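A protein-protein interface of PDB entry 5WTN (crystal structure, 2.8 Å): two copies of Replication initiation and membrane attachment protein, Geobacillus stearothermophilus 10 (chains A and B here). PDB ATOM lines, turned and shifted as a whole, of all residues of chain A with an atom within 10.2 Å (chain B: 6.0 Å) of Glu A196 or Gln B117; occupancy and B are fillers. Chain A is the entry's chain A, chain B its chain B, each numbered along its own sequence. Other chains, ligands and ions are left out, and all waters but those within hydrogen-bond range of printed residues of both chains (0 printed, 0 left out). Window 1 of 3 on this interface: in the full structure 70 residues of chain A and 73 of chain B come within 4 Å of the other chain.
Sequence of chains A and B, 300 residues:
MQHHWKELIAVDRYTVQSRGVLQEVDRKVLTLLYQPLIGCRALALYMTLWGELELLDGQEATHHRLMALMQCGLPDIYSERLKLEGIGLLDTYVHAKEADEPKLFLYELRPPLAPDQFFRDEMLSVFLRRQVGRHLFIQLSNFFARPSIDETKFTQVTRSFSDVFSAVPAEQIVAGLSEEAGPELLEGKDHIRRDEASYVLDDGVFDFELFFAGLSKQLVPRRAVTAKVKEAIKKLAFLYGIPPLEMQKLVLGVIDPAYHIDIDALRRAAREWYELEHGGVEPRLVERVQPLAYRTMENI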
ATOM      1  N   ARG A  19     -21.633  28.829 -28.027  1.00  0.00           N
ATOM      2  CA  ARG A  19     -20.660  28.795 -26.942  1.00  0.00           C
ATOM      3  C   ARG A  19     -19.397  28.034 -27.353  1.00  0.00           C
ATOM      4  O   ARG A  19     -18.439  27.911 -26.577  1.00  0.00           O
ATOM      5  CB  ARG A  19     -21.247  28.349 -25.584  1.00  0.00           C
ATOM      6  CG  ARG A  19     -22.455  27.414 -25.631  1.00  0.00           C
ATOM      7  CD  ARG A  19     -23.770  28.105 -25.228  1.00  0.00           C
ATOM      8  NE  ARG A  19     -24.084  29.245 -26.094  1.00  0.00           N
ATOM      9  CZ  ARG A  19     -24.062  30.521 -25.699  1.00  0.00           C
ATOM     10  NH1 ARG A  19     -23.764  30.830 -24.435  1.00  0.00           N
ATOM     11  NH2 ARG A  19     -24.354  31.488 -26.563  1.00  0.00           N
ATOM     12  N   ALA A 114     -16.088  15.076 -32.643  1.00  0.00           N
ATOM     13  CA  ALA A 114     -14.683  14.815 -32.945  1.00  0.00           C
ATOM     14  C   ALA A 114     -14.690  13.525 -33.734  1.00  0.00           C
ATOM     15  O   ALA A 114     -15.529  12.656 -33.500  1.00  0.00           O
ATOM     16  CB  ALA A 114     -13.892  14.670 -31.692  1.00  0.00           C
ATOM     17  N   ASP A 116     -13.213  10.759 -33.552  1.00  0.00           N
ATOM     18  CA  ASP A 116     -13.355   9.540 -32.768  1.00  0.00           C
ATOM     19  C   ASP A 116     -14.810   9.311 -32.314  1.00  0.00           C
ATOM     20  O   ASP A 116     -15.327   8.208 -32.410  1.00  0.00           O
ATOM     21  CB  ASP A 116     -12.378   9.510 -31.585  1.00  0.00           C
ATOM     22  CG  ASP A 116     -12.844  10.363 -30.407  1.00  0.00           C
ATOM     23  OD1 ASP A 116     -12.961   9.819 -29.296  1.00  0.00           O
ATOM     24  OD2 ASP A 116     -13.078  11.585 -30.569  1.00  0.00           O
ATOM     25  N   GLN A 117     -15.475  10.361 -31.848  1.00  0.00           N
ATOM     26  CA  GLN A 117     -16.845  10.252 -31.412  1.00  0.00           C
ATOM     27  C   GLN A 117     -17.740   9.869 -32.589  1.00  0.00           C
ATOM     28  O   GLN A 117     -18.726   9.122 -32.445  1.00  0.00           O
ATOM     29  CB  GLN A 117     -17.295  11.582 -30.837  1.00  0.00           C
ATOM     30  CG  GLN A 117     -16.500  12.068 -29.633  1.00  0.00           C
ATOM     31  CD  GLN A 117     -16.922  13.465 -29.143  1.00  0.00           C
ATOM     32  OE1 GLN A 117     -16.937  14.453 -29.912  1.00  0.00           O
ATOM     33  NE2 GLN A 117     -17.267  13.552 -27.854  1.00  0.00           N
ATOM     34  N   ARG A 193      -8.925  12.878 -31.593  1.00  0.00           N
ATOM     35  CA  ARG A 193      -9.840  13.099 -30.479  1.00  0.00           C
ATOM     36  C   ARG A 193      -9.346  14.280 -29.671  1.00  0.00           C
ATOM     37  O   ARG A 193      -8.206  14.718 -29.840  1.00  0.00           O
ATOM     38  CB  ARG A 193      -9.904  11.854 -29.596  1.00  0.00           C
ATOM     39  CG  ARG A 193      -8.663  11.622 -28.771  1.00  0.00           C
ATOM     40  CD  ARG A 193      -8.655  10.223 -28.182  1.00  0.00           C
ATOM     41  NE  ARG A 193      -7.559  10.055 -27.230  1.00  0.00           N
ATOM     42  CZ  ARG A 193      -7.115   8.882 -26.795  1.00  0.00           C
ATOM     43  NH1 ARG A 193      -7.666   7.760 -27.232  1.00  0.00           N
ATOM     44  NH2 ARG A 193      -6.113   8.834 -25.924  1.00  0.00           N
ATOM     45  N   ARG A 194     -10.159  14.783 -28.753  1.00  0.00           N
ATOM     46  CA  ARG A 194      -9.715  15.899 -27.925  1.00  0.00           C
ATOM     47  C   ARG A 194      -9.282  15.457 -26.527  1.00  0.00           C
ATOM     48  O   ARG A 194     -10.108  15.395 -25.617  1.00  0.00           O
ATOM     49  CB  ARG A 194     -10.816  16.957 -27.821  1.00  0.00           C
ATOM     50  CG  ARG A 194     -12.187  16.396 -27.483  1.00  0.00           C
ATOM     51  CD  ARG A 194     -13.194  17.507 -27.237  1.00  0.00           C
ATOM     52  NE  ARG A 194     -14.175  17.605 -28.315  1.00  0.00           N
ATOM     53  CZ  ARG A 194     -15.472  17.826 -28.127  1.00  0.00           C
ATOM     54  NH1 ARG A 194     -15.950  17.975 -26.898  1.00  0.00           N
ATOM     55  NH2 ARG A 194     -16.292  17.900 -29.165  1.00  0.00           N
ATOM     56  N   ASP A 195      -7.995  15.159 -26.344  1.00  0.00           N
ATOM     57  CA  ASP A 195      -7.522  14.830 -25.007  1.00  0.00           C
ATOM     58  C   ASP A 195      -6.987  16.121 -24.422  1.00  0.00           C
ATOM     59  O   ASP A 195      -5.848  16.521 -24.713  1.00  0.00           O
ATOM     60  CB  ASP A 195      -6.377  13.817 -25.077  1.00  0.00           C
ATOM     61  CG  ASP A 195      -6.858  12.386 -25.161  1.00  0.00           C
ATOM     62  OD1 ASP A 195      -6.070  11.537 -25.643  1.00  0.00           O
ATOM     63  OD2 ASP A 195      -8.008  12.111 -24.743  1.00  0.00           O
ATOM     64  N   GLU A 196      -7.805  16.777 -23.606  1.00  0.00           N
ATOM     65  CA  GLU A 196      -7.411  18.021 -22.960  1.00  0.00           C
ATOM     66  C   GLU A 196      -6.296  17.765 -21.956  1.00  0.00           C
ATOM     67  O   GLU A 196      -6.188  16.671 -21.402  1.00  0.00           O
ATOM     68  CB  GLU A 196      -8.609  18.669 -22.265  1.00  0.00           C
ATOM     69  CG  GLU A 196      -9.391  17.724 -21.367  1.00  0.00           C
ATOM     70  CD  GLU A 196     -10.680  17.246 -22.005  1.00  0.00           C
ATOM     71  OE1 GLU A 196     -11.675  17.063 -21.272  1.00  0.00           O
ATOM     72  OE2 GLU A 196     -10.699  17.053 -23.238  1.00  0.00           O
ATOM     73  N   ALA A 197      -5.468  18.777 -21.726  1.00  0.00           N
ATOM     74  CA  ALA A 197      -4.343  18.647 -20.802  1.00  0.00           C
ATOM     75  C   ALA A 197      -4.804  18.520 -19.349  1.00  0.00           C
ATOM     76  O   ALA A 197      -5.396  19.443 -18.772  1.00  0.00           O
ATOM     77  CB  ALA A 197      -3.423  19.877 -20.946  1.00  0.00           C
ATOM     78  N   SER A 198      -4.464  17.411 -18.716  1.00  0.00           N
ATOM     79  CA  SER A 198      -4.843  17.295 -17.335  1.00  0.00           C
ATOM     80  C   SER A 198      -3.547  17.280 -16.592  1.00  0.00           C
ATOM     81  O   SER A 198      -2.849  16.269 -16.590  1.00  0.00           O
ATOM     82  CB  SER A 198      -5.613  15.996 -17.116  1.00  0.00           C
ATOM     83  OG  SER A 198      -6.661  15.879 -18.066  1.00  0.00           O
ATOM     84  N   TYR A 199      -3.219  18.387 -15.939  1.00  0.00           N
ATOM     85  CA  TYR A 199      -2.029  18.379 -15.111  1.00  0.00           C
ATOM     86  C   TYR A 199      -2.325  17.481 -13.906  1.00  0.00           C
ATOM     87  O   TYR A 199      -3.505  17.243 -13.585  1.00  0.00           O
ATOM     88  CB  TYR A 199      -1.583  19.799 -14.717  1.00  0.00           C
ATOM     89  CG  TYR A 199      -2.477  20.547 -13.756  1.00  0.00           C
ATOM     90  CD1 TYR A 199      -2.550  20.186 -12.421  1.00  0.00           C
ATOM     91  CD2 TYR A 199      -3.208  21.653 -14.170  1.00  0.00           C
ATOM     92  CE1 TYR A 199      -3.357  20.875 -11.532  1.00  0.00           C
ATOM     93  CE2 TYR A 199      -4.011  22.358 -13.281  1.00  0.00           C
ATOM     94  CZ  TYR A 199      -4.083  21.959 -11.963  1.00  0.00           C
ATOM     95  OH  TYR A 199      -4.883  22.635 -11.066  1.00  0.00           O
ATOM     96  N   VAL A 200      -1.281  16.957 -13.264  1.00  0.00           N
ATOM     97  CA  VAL A 200      -1.480  16.140 -12.071  1.00  0.00           C
ATOM     98  C   VAL A 200      -0.595  16.620 -10.941  1.00  0.00           C
ATOM     99  O   VAL A 200       0.432  17.259 -11.193  1.00  0.00           O
ATOM    100  CB  VAL A 200      -1.219  14.643 -12.323  1.00  0.00           C
ATOM    101  CG1 VAL A 200      -2.408  14.011 -13.027  1.00  0.00           C
ATOM    102  CG2 VAL A 200       0.053  14.447 -13.118  1.00  0.00           C
ATOM    103  N   GLU A 231      -9.145  14.912  -5.411  1.00  0.00           N
ATOM    104  CA  GLU A 231      -8.426  15.705  -6.393  1.00  0.00           C
ATOM    105  C   GLU A 231      -8.502  17.178  -5.989  1.00  0.00           C
ATOM    106  O   GLU A 231      -7.515  17.905  -6.064  1.00  0.00           O
ATOM    107  CB  GLU A 231      -9.036  15.471  -7.781  1.00  0.00           C
ATOM    108  CG  GLU A 231      -8.383  16.225  -8.940  1.00  0.00           C
ATOM    109  CD  GLU A 231      -9.158  16.062 -10.258  1.00  0.00           C
ATOM    110  OE1 GLU A 231      -8.933  16.874 -11.193  1.00  0.00           O
ATOM    111  OE2 GLU A 231      -9.989  15.122 -10.363  1.00  0.00           O
ATOM    112  N   LYS A 235      -5.458  20.007  -4.730  1.00  0.00           N
ATOM    113  CA  LYS A 235      -5.154  21.277  -5.380  1.00  0.00           C
ATOM    114  C   LYS A 235      -5.239  22.393  -4.370  1.00  0.00           C
ATOM    115  O   LYS A 235      -4.444  23.328  -4.404  1.00  0.00           O
ATOM    116  CB  LYS A 235      -6.110  21.554  -6.539  1.00  0.00           C
ATOM    117  CG  LYS A 235      -6.264  20.409  -7.516  1.00  0.00           C
ATOM    118  CD  LYS A 235      -6.705  20.924  -8.880  1.00  0.00           C
ATOM    119  CE  LYS A 235      -6.859  19.798  -9.899  1.00  0.00           C
ATOM    120  NZ  LYS A 235      -7.646  20.265 -11.079  1.00  0.00           N
ATOM    121  N   ARG A 267     -13.963  25.041  -1.849  1.00  0.00           N
ATOM    122  CA  ARG A 267     -13.101  26.029  -2.492  1.00  0.00           C
ATOM    123  C   ARG A 267     -13.204  27.397  -1.830  1.00  0.00           C
ATOM    124  O   ARG A 267     -12.186  28.038  -1.575  1.00  0.00           O
ATOM    125  CB  ARG A 267     -13.391  26.135  -4.005  1.00  0.00           C
ATOM    126  CG  ARG A 267     -12.885  24.932  -4.837  1.00  0.00           C
ATOM    127  CD  ARG A 267     -13.150  25.049  -6.356  1.00  0.00           C
ATOM    128  NE  ARG A 267     -12.569  26.247  -6.986  1.00  0.00           N
ATOM    129  CZ  ARG A 267     -12.565  26.471  -8.304  1.00  0.00           C
ATOM    130  NH1 ARG A 267     -13.094  25.567  -9.126  1.00  0.00           N
ATOM    131  NH2 ARG A 267     -12.025  27.587  -8.808  1.00  0.00           N
ATOM    132  N   GLY B  88       0.866  20.300 -18.132  1.00  0.00           N
ATOM    133  CA  GLY B  88       0.033  19.328 -18.823  1.00  0.00           C
ATOM    134  C   GLY B  88       0.000  19.338 -20.351  1.00  0.00           C
ATOM    135  O   GLY B  88      -0.674  18.503 -20.969  1.00  0.00           O
ATOM    136  N   ARG B 110      -0.234  17.518 -26.054  1.00  0.00           N
ATOM    137  CA  ARG B 110      -1.587  17.571 -25.511  1.00  0.00           C
ATOM    138  C   ARG B 110      -2.126  18.985 -25.648  1.00  0.00           C
ATOM    139  O   ARG B 110      -1.509  19.937 -25.172  1.00  0.00           O
ATOM    140  CB  ARG B 110      -1.595  17.140 -24.045  1.00  0.00           C
ATOM    141  CG  ARG B 110      -1.415  15.645 -23.836  1.00  0.00           C
ATOM    142  CD  ARG B 110      -2.755  14.931 -23.775  1.00  0.00           C
ATOM    143  NE  ARG B 110      -2.769  13.880 -22.762  1.00  0.00           N
ATOM    144  CZ  ARG B 110      -3.584  13.863 -21.714  1.00  0.00           C
ATOM    145  NH1 ARG B 110      -4.458  14.844 -21.535  1.00  0.00           N
ATOM    146  NH2 ARG B 110      -3.527  12.866 -20.842  1.00  0.00           N
ATOM    147  N   PRO B 111      -3.273  19.129 -26.305  1.00  0.00           N
ATOM    148  CA  PRO B 111      -3.802  20.473 -26.566  1.00  0.00           C
ATOM    149  C   PRO B 111      -4.166  21.134 -25.245  1.00  0.00           C
ATOM    150  O   PRO B 111      -4.351  20.430 -24.231  1.00  0.00           O
ATOM    151  CB  PRO B 111      -5.022  20.197 -27.424  1.00  0.00           C
ATOM    152  CG  PRO B 111      -4.726  18.813 -28.033  1.00  0.00           C
ATOM    153  CD  PRO B 111      -4.116  18.082 -26.886  1.00  0.00           C
ATOM    154  N   PRO B 112      -4.204  22.475 -25.233  1.00  0.00           N
ATOM    155  CA  PRO B 112      -4.544  23.216 -24.016  1.00  0.00           C
ATOM    156  C   PRO B 112      -5.954  22.938 -23.523  1.00  0.00           C
ATOM    157  O   PRO B 112      -6.819  22.531 -24.291  1.00  0.00           O
ATOM    158  CB  PRO B 112      -4.411  24.687 -24.434  1.00  0.00           C
ATOM    159  CG  PRO B 112      -4.180  24.693 -25.886  1.00  0.00           C
ATOM    160  CD  PRO B 112      -3.709  23.349 -26.303  1.00  0.00           C
ATOM    161  N   LEU B 113      -6.195  23.157 -22.240  1.00  0.00           N
ATOM    162  CA  LEU B 113      -7.566  23.211 -21.773  1.00  0.00           C
ATOM    163  C   LEU B 113      -8.351  24.233 -22.588  1.00  0.00           C
ATOM    164  O   LEU B 113      -7.795  25.210 -23.088  1.00  0.00           O
ATOM    165  CB  LEU B 113      -7.606  23.632 -20.324  1.00  0.00           C
ATOM    166  CG  LEU B 113      -6.975  22.625 -19.397  1.00  0.00           C
ATOM    167  CD1 LEU B 113      -7.062  23.140 -17.973  1.00  0.00           C
ATOM    168  CD2 LEU B 113      -7.698  21.320 -19.581  1.00  0.00           C
ATOM    169  N   ALA B 114      -9.642  23.973 -22.769  1.00  0.00           N
ATOM    170  CA  ALA B 114     -10.518  24.956 -23.378  1.00  0.00           C
ATOM    171  C   ALA B 114     -10.707  26.061 -22.361  1.00  0.00           C
ATOM    172  O   ALA B 114     -10.503  25.844 -21.170  1.00  0.00           O
ATOM    173  CB  ALA B 114     -11.809  24.340 -23.712  1.00  0.00           C
ATOM    174  N   PRO B 115     -11.086  27.257 -22.817  1.00  0.00           N
ATOM    175  CA  PRO B 115     -11.254  28.330 -21.836  1.00  0.00           C
ATOM    176  C   PRO B 115     -12.155  28.008 -20.615  1.00  0.00           C
ATOM    177  O   PRO B 115     -11.708  28.300 -19.491  1.00  0.00           O
ATOM    178  CB  PRO B 115     -11.828  29.465 -22.673  1.00  0.00           C
ATOM    179  CG  PRO B 115     -11.271  29.227 -24.024  1.00  0.00           C
ATOM    180  CD  PRO B 115     -11.207  27.744 -24.202  1.00  0.00           C
ATOM    181  N   ASP B 116     -13.344  27.420 -20.775  1.00  0.00           N
ATOM    182  CA  ASP B 116     -14.152  27.143 -19.566  1.00  0.00           C
ATOM    183  C   ASP B 116     -13.429  26.257 -18.554  1.00  0.00           C
ATOM    184  O   ASP B 116     -13.470  26.539 -17.368  1.00  0.00           O
ATOM    185  CB  ASP B 116     -15.553  26.574 -19.863  1.00  0.00           C
ATOM    186  CG  ASP B 116     -15.522  25.100 -20.281  1.00  0.00           C
ATOM    187  OD1 ASP B 116     -14.689  24.719 -21.154  1.00  0.00           O
ATOM    188  OD2 ASP B 116     -16.349  24.320 -19.759  1.00  0.00           O
ATOM    189  N   GLN B 117     -12.760  25.204 -19.020  1.00  0.00           N
ATOM    190  CA  GLN B 117     -11.997  24.334 -18.128  1.00  0.00           C
ATOM    191  C   GLN B 117     -10.830  25.078 -17.456  1.00  0.00           C
ATOM    192  O   GLN B 117     -10.470  24.793 -16.319  1.00  0.00           O
ATOM    193  CB  GLN B 117     -11.443  23.121 -18.868  1.00  0.00           C
ATOM    194  CG  GLN B 117     -12.458  22.186 -19.463  1.00  0.00           C
ATOM    195  CD  GLN B 117     -11.792  21.061 -20.267  1.00  0.00           C
ATOM    196  OE1 GLN B 117     -11.187  21.312 -21.320  1.00  0.00           O
ATOM    197  NE2 GLN B 117     -11.910  19.811 -19.775  1.00  0.00           N
ATOM    198  N   PHE B 118     -10.232  26.022 -18.159  1.00  0.00           N
ATOM    199  CA  PHE B 118      -9.100  26.707 -17.590  1.00  0.00           C
ATOM    200  C   PHE B 118      -9.531  27.525 -16.395  1.00  0.00           C
ATOM    201  O   PHE B 118      -9.025  27.340 -15.279  1.00  0.00           O
ATOM    202  CB  PHE B 118      -8.449  27.607 -18.637  1.00  0.00           C
ATOM    203  CG  PHE B 118      -7.187  28.249 -18.171  1.00  0.00           C
ATOM    204  CD1 PHE B 118      -5.967  27.648 -18.426  1.00  0.00           C
ATOM    205  CD2 PHE B 118      -7.214  29.455 -17.468  1.00  0.00           C
ATOM    206  CE1 PHE B 118      -4.786  28.236 -18.004  1.00  0.00           C
ATOM    207  CE2 PHE B 118      -6.022  30.053 -17.026  1.00  0.00           C
ATOM    208  CZ  PHE B 118      -4.814  29.446 -17.296  1.00  0.00           C
ATOM    209  N   PHE B 119     -10.482  28.420 -16.634  1.00  0.00           N
ATOM    210  CA  PHE B 119     -10.996  29.299 -15.589  1.00  0.00           C
ATOM    211  C   PHE B 119     -11.685  28.565 -14.450  1.00  0.00           C
ATOM    212  O   PHE B 119     -11.731  29.054 -13.327  1.00  0.00           O
ATOM    213  CB  PHE B 119     -11.946  30.320 -16.188  1.00  0.00           C
ATOM    214  CG  PHE B 119     -11.260  31.425 -16.927  1.00  0.00           C
ATOM    215  CD1 PHE B 119     -10.647  32.469 -16.239  1.00  0.00           C
ATOM    216  CD2 PHE B 119     -11.231  31.435 -18.304  1.00  0.00           C
ATOM    217  CE1 PHE B 119     -10.014  33.498 -16.919  1.00  0.00           C
ATOM    218  CE2 PHE B 119     -10.600  32.466 -18.978  1.00  0.00           C
ATOM    219  CZ  PHE B 119      -9.995  33.490 -18.289  1.00  0.00           C
ATOM    220  N   ARG B 120     -12.210  27.384 -14.730  1.00  0.00           N
ATOM    221  CA  ARG B 120     -12.869  26.613 -13.687  1.00  0.00           C
ATOM    222  C   ARG B 120     -11.892  25.938 -12.756  1.00  0.00           C
ATOM    223  O   ARG B 120     -12.235  25.585 -11.624  1.00  0.00           O
ATOM    224  CB  ARG B 120     -13.835  25.596 -14.276  1.00  0.00           C
ATOM    225  CG  ARG B 120     -15.241  26.152 -14.361  1.00  0.00           C
ATOM    226  CD  ARG B 120     -16.266  25.101 -14.014  1.00  0.00           C
ATOM    227  NE  ARG B 120     -16.113  23.951 -14.897  1.00  0.00           N
ATOM    228  CZ  ARG B 120     -16.702  23.842 -16.085  1.00  0.00           C
ATOM    229  NH1 ARG B 120     -17.502  24.824 -16.519  1.00  0.00           N
ATOM    230  NH2 ARG B 120     -16.491  22.754 -16.829  1.00  0.00           N
ATOM    231  N   ASP B 121     -10.671  25.768 -13.242  1.00  0.00           N
ATOM    232  CA  ASP B 121      -9.626  25.158 -12.451  1.00  0.00           C
ATOM    233  C   ASP B 121      -9.206  26.030 -11.272  1.00  0.00           C
ATOM    234  O   ASP B 121      -8.949  27.226 -11.453  1.00  0.00           O
ATOM    235  CB  ASP B 121      -8.411  24.862 -13.315  1.00  0.00           C
ATOM    236  CG  ASP B 121      -7.387  24.043 -12.586  1.00  0.00           C
ATOM    237  OD1 ASP B 121      -6.416  24.637 -12.060  1.00  0.00           O
ATOM    238  OD2 ASP B 121      -7.582  22.810 -12.498  1.00  0.00           O
ATOM    239  N   LEU B 124      -5.098  27.280 -11.670  1.00  0.00           N
ATOM    240  CA  LEU B 124      -4.698  28.003 -12.862  1.00  0.00           C
ATOM    241  C   LEU B 124      -5.261  29.406 -12.852  1.00  0.00           C
ATOM    242  O   LEU B 124      -4.563  30.384 -13.143  1.00  0.00           O
ATOM    243  CB  LEU B 124      -5.114  27.260 -14.121  1.00  0.00           C
ATOM    244  CG  LEU B 124      -4.506  25.860 -14.300  1.00  0.00           C
ATOM    245  CD1 LEU B 124      -4.914  25.189 -15.597  1.00  0.00           C
ATOM    246  CD2 LEU B 124      -3.009  25.954 -14.226  1.00  0.00           C
ATOM    247  N   ILE B 192     -16.278  30.046 -23.258  1.00  0.00           N
ATOM    248  CA  ILE B 192     -16.162  29.167 -24.420  1.00  0.00           C
ATOM    249  C   ILE B 192     -15.782  27.749 -24.012  1.00  0.00           C
ATOM    250  O   ILE B 192     -14.828  27.548 -23.235  1.00  0.00           O
ATOM    251  CB  ILE B 192     -15.093  29.693 -25.390  1.00  0.00           C
ATOM    252  CG1 ILE B 192     -15.575  30.989 -26.051  1.00  0.00           C
ATOM    253  CG2 ILE B 192     -14.773  28.650 -26.443  1.00  0.00           C
ATOM    254  CD1 ILE B 192     -14.529  31.664 -26.905  1.00  0.00           C
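Positions printed for both chains: 114, 116 and 117.
The guanidinium group (NE) of Arg A193 lies within salt-bridge range of the side-chain carboxylate (OD1) of Asp A195 (2.6 Å). The side-chain hydroxyl of Ser A198 lies within hydrogen-bond range of the backbone carbonyl oxygen of Glu A196 (3.5 Å). The side-chain amino group (NZ) of Lys A235 lies within salt-bridge range of the side-chain carboxylate (OE1) of Glu A231, 3.6 Å away. The side-chain carboxylate (OD2) of Asp B116 is in salt-bridge range of the guanidinium group (NH2) of Arg B120 (3.3 Å). O of Ile B192 is in hydrogen-bond range of N of Asp B116. The side-chain carboxylate (OD1) of Asp B121 sits at hydrogen-bond distance from the backbone NH (N) of Leu B124 (3.0 Å).
Printed residues of chain B within 4 Å of Arg A19: Ile B192. Arg A193 touches none of the printed residues of chain B. Printed residues of chain B within 4 Å of Asp A195: Arg B110 (3.6 Å) and Pro B111 (3.2 Å). Printed residues of chain B within 4 Å of Glu A196: Arg B110, Leu B113 and Gln B117. Of the printed residues of chain B, Lys A235 touches Asp B121. Leu B113 touches just these residues of chain A: Glu A196 (3.9 Å) and Ala A197 (3.1 Å). No residue of chain A comes within 4 Å of Ala B114. No residue of chain A comes within 4 Å of Asp B116. Arg B120 touches just one residue of chain A: Arg A267. The nearest printed residue of chain B that does not touch Glu A196 is Pro B111 (4.01 Å). The nearest residue of chain A that does not touch Gln B117 is Ala A197 (6.3 Å). The nearest printed residue of chain B that does not touch Arg A19 is Asp B116 (7.3 Å).
The guanidinium group of Arg B110 sits at hydrogen-bond distance from the backbone carbonyl oxygen of Glu A196, 2.5 Å away. The side-chain carboxylate of Glu A196 sits at hydrogen-bond distance from the side-chain amide nitrogen of Gln B117, 3.1 Å away. The backbone carbonyl oxygen (O) of Pro B111 sits at hydrogen-bond distance from the backbone NH (N) of Ala A197, 3.2 Å away. OH of Tyr A199 lies within hydrogen-bond range of OD1 of Asp B121 (2.7 Å). The side-chain amino group of Lys A235 lies within salt-bridge range of the side-chain carboxylate of Asp B121. O of Arg B120 is in hydrogen-bond range of NH1 of Arg A267, 2.6 Å away.
Among the printed residues, pairs that only touch across the chains: Ala A197 with Gly B88 (3.1 Å), Ala A197 with Leu B113 (3.1 Å), Asp A195 with Pro B111 (3.2 Å), Arg A19 with Ile B192 (3.4 Å), Asp A195 with Arg B110 (3.6 Å), Tyr A199 with Leu B124 (3.7 Å), Ser A198 with Arg B110 (3.8 Å), Ala A197 with Arg B110 (3.9 Å) and Glu A196 with Leu B113 (3.9 Å).
Of the 15 printed residues of chain A, 8 touch a printed residue of chain B. Printed residues of chain A that touch a printed residue of chain B: Arg A19, Asp A195, Glu A196, Ala A197, Ser A198, Tyr A199, Lys A235 and Arg A267. Hydrophobic or aromatic side chains of chain A within 4 Å of the printed part of chain B: Ala A197 and Tyr A199. Along chain A the printed residues that touch a printed residue of chain B span positions 19 to 267. Of the 15 printed residues of chain B, 9 touch a printed residue of chain A. Among the printed residues, 15 pairs touch across the chains.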
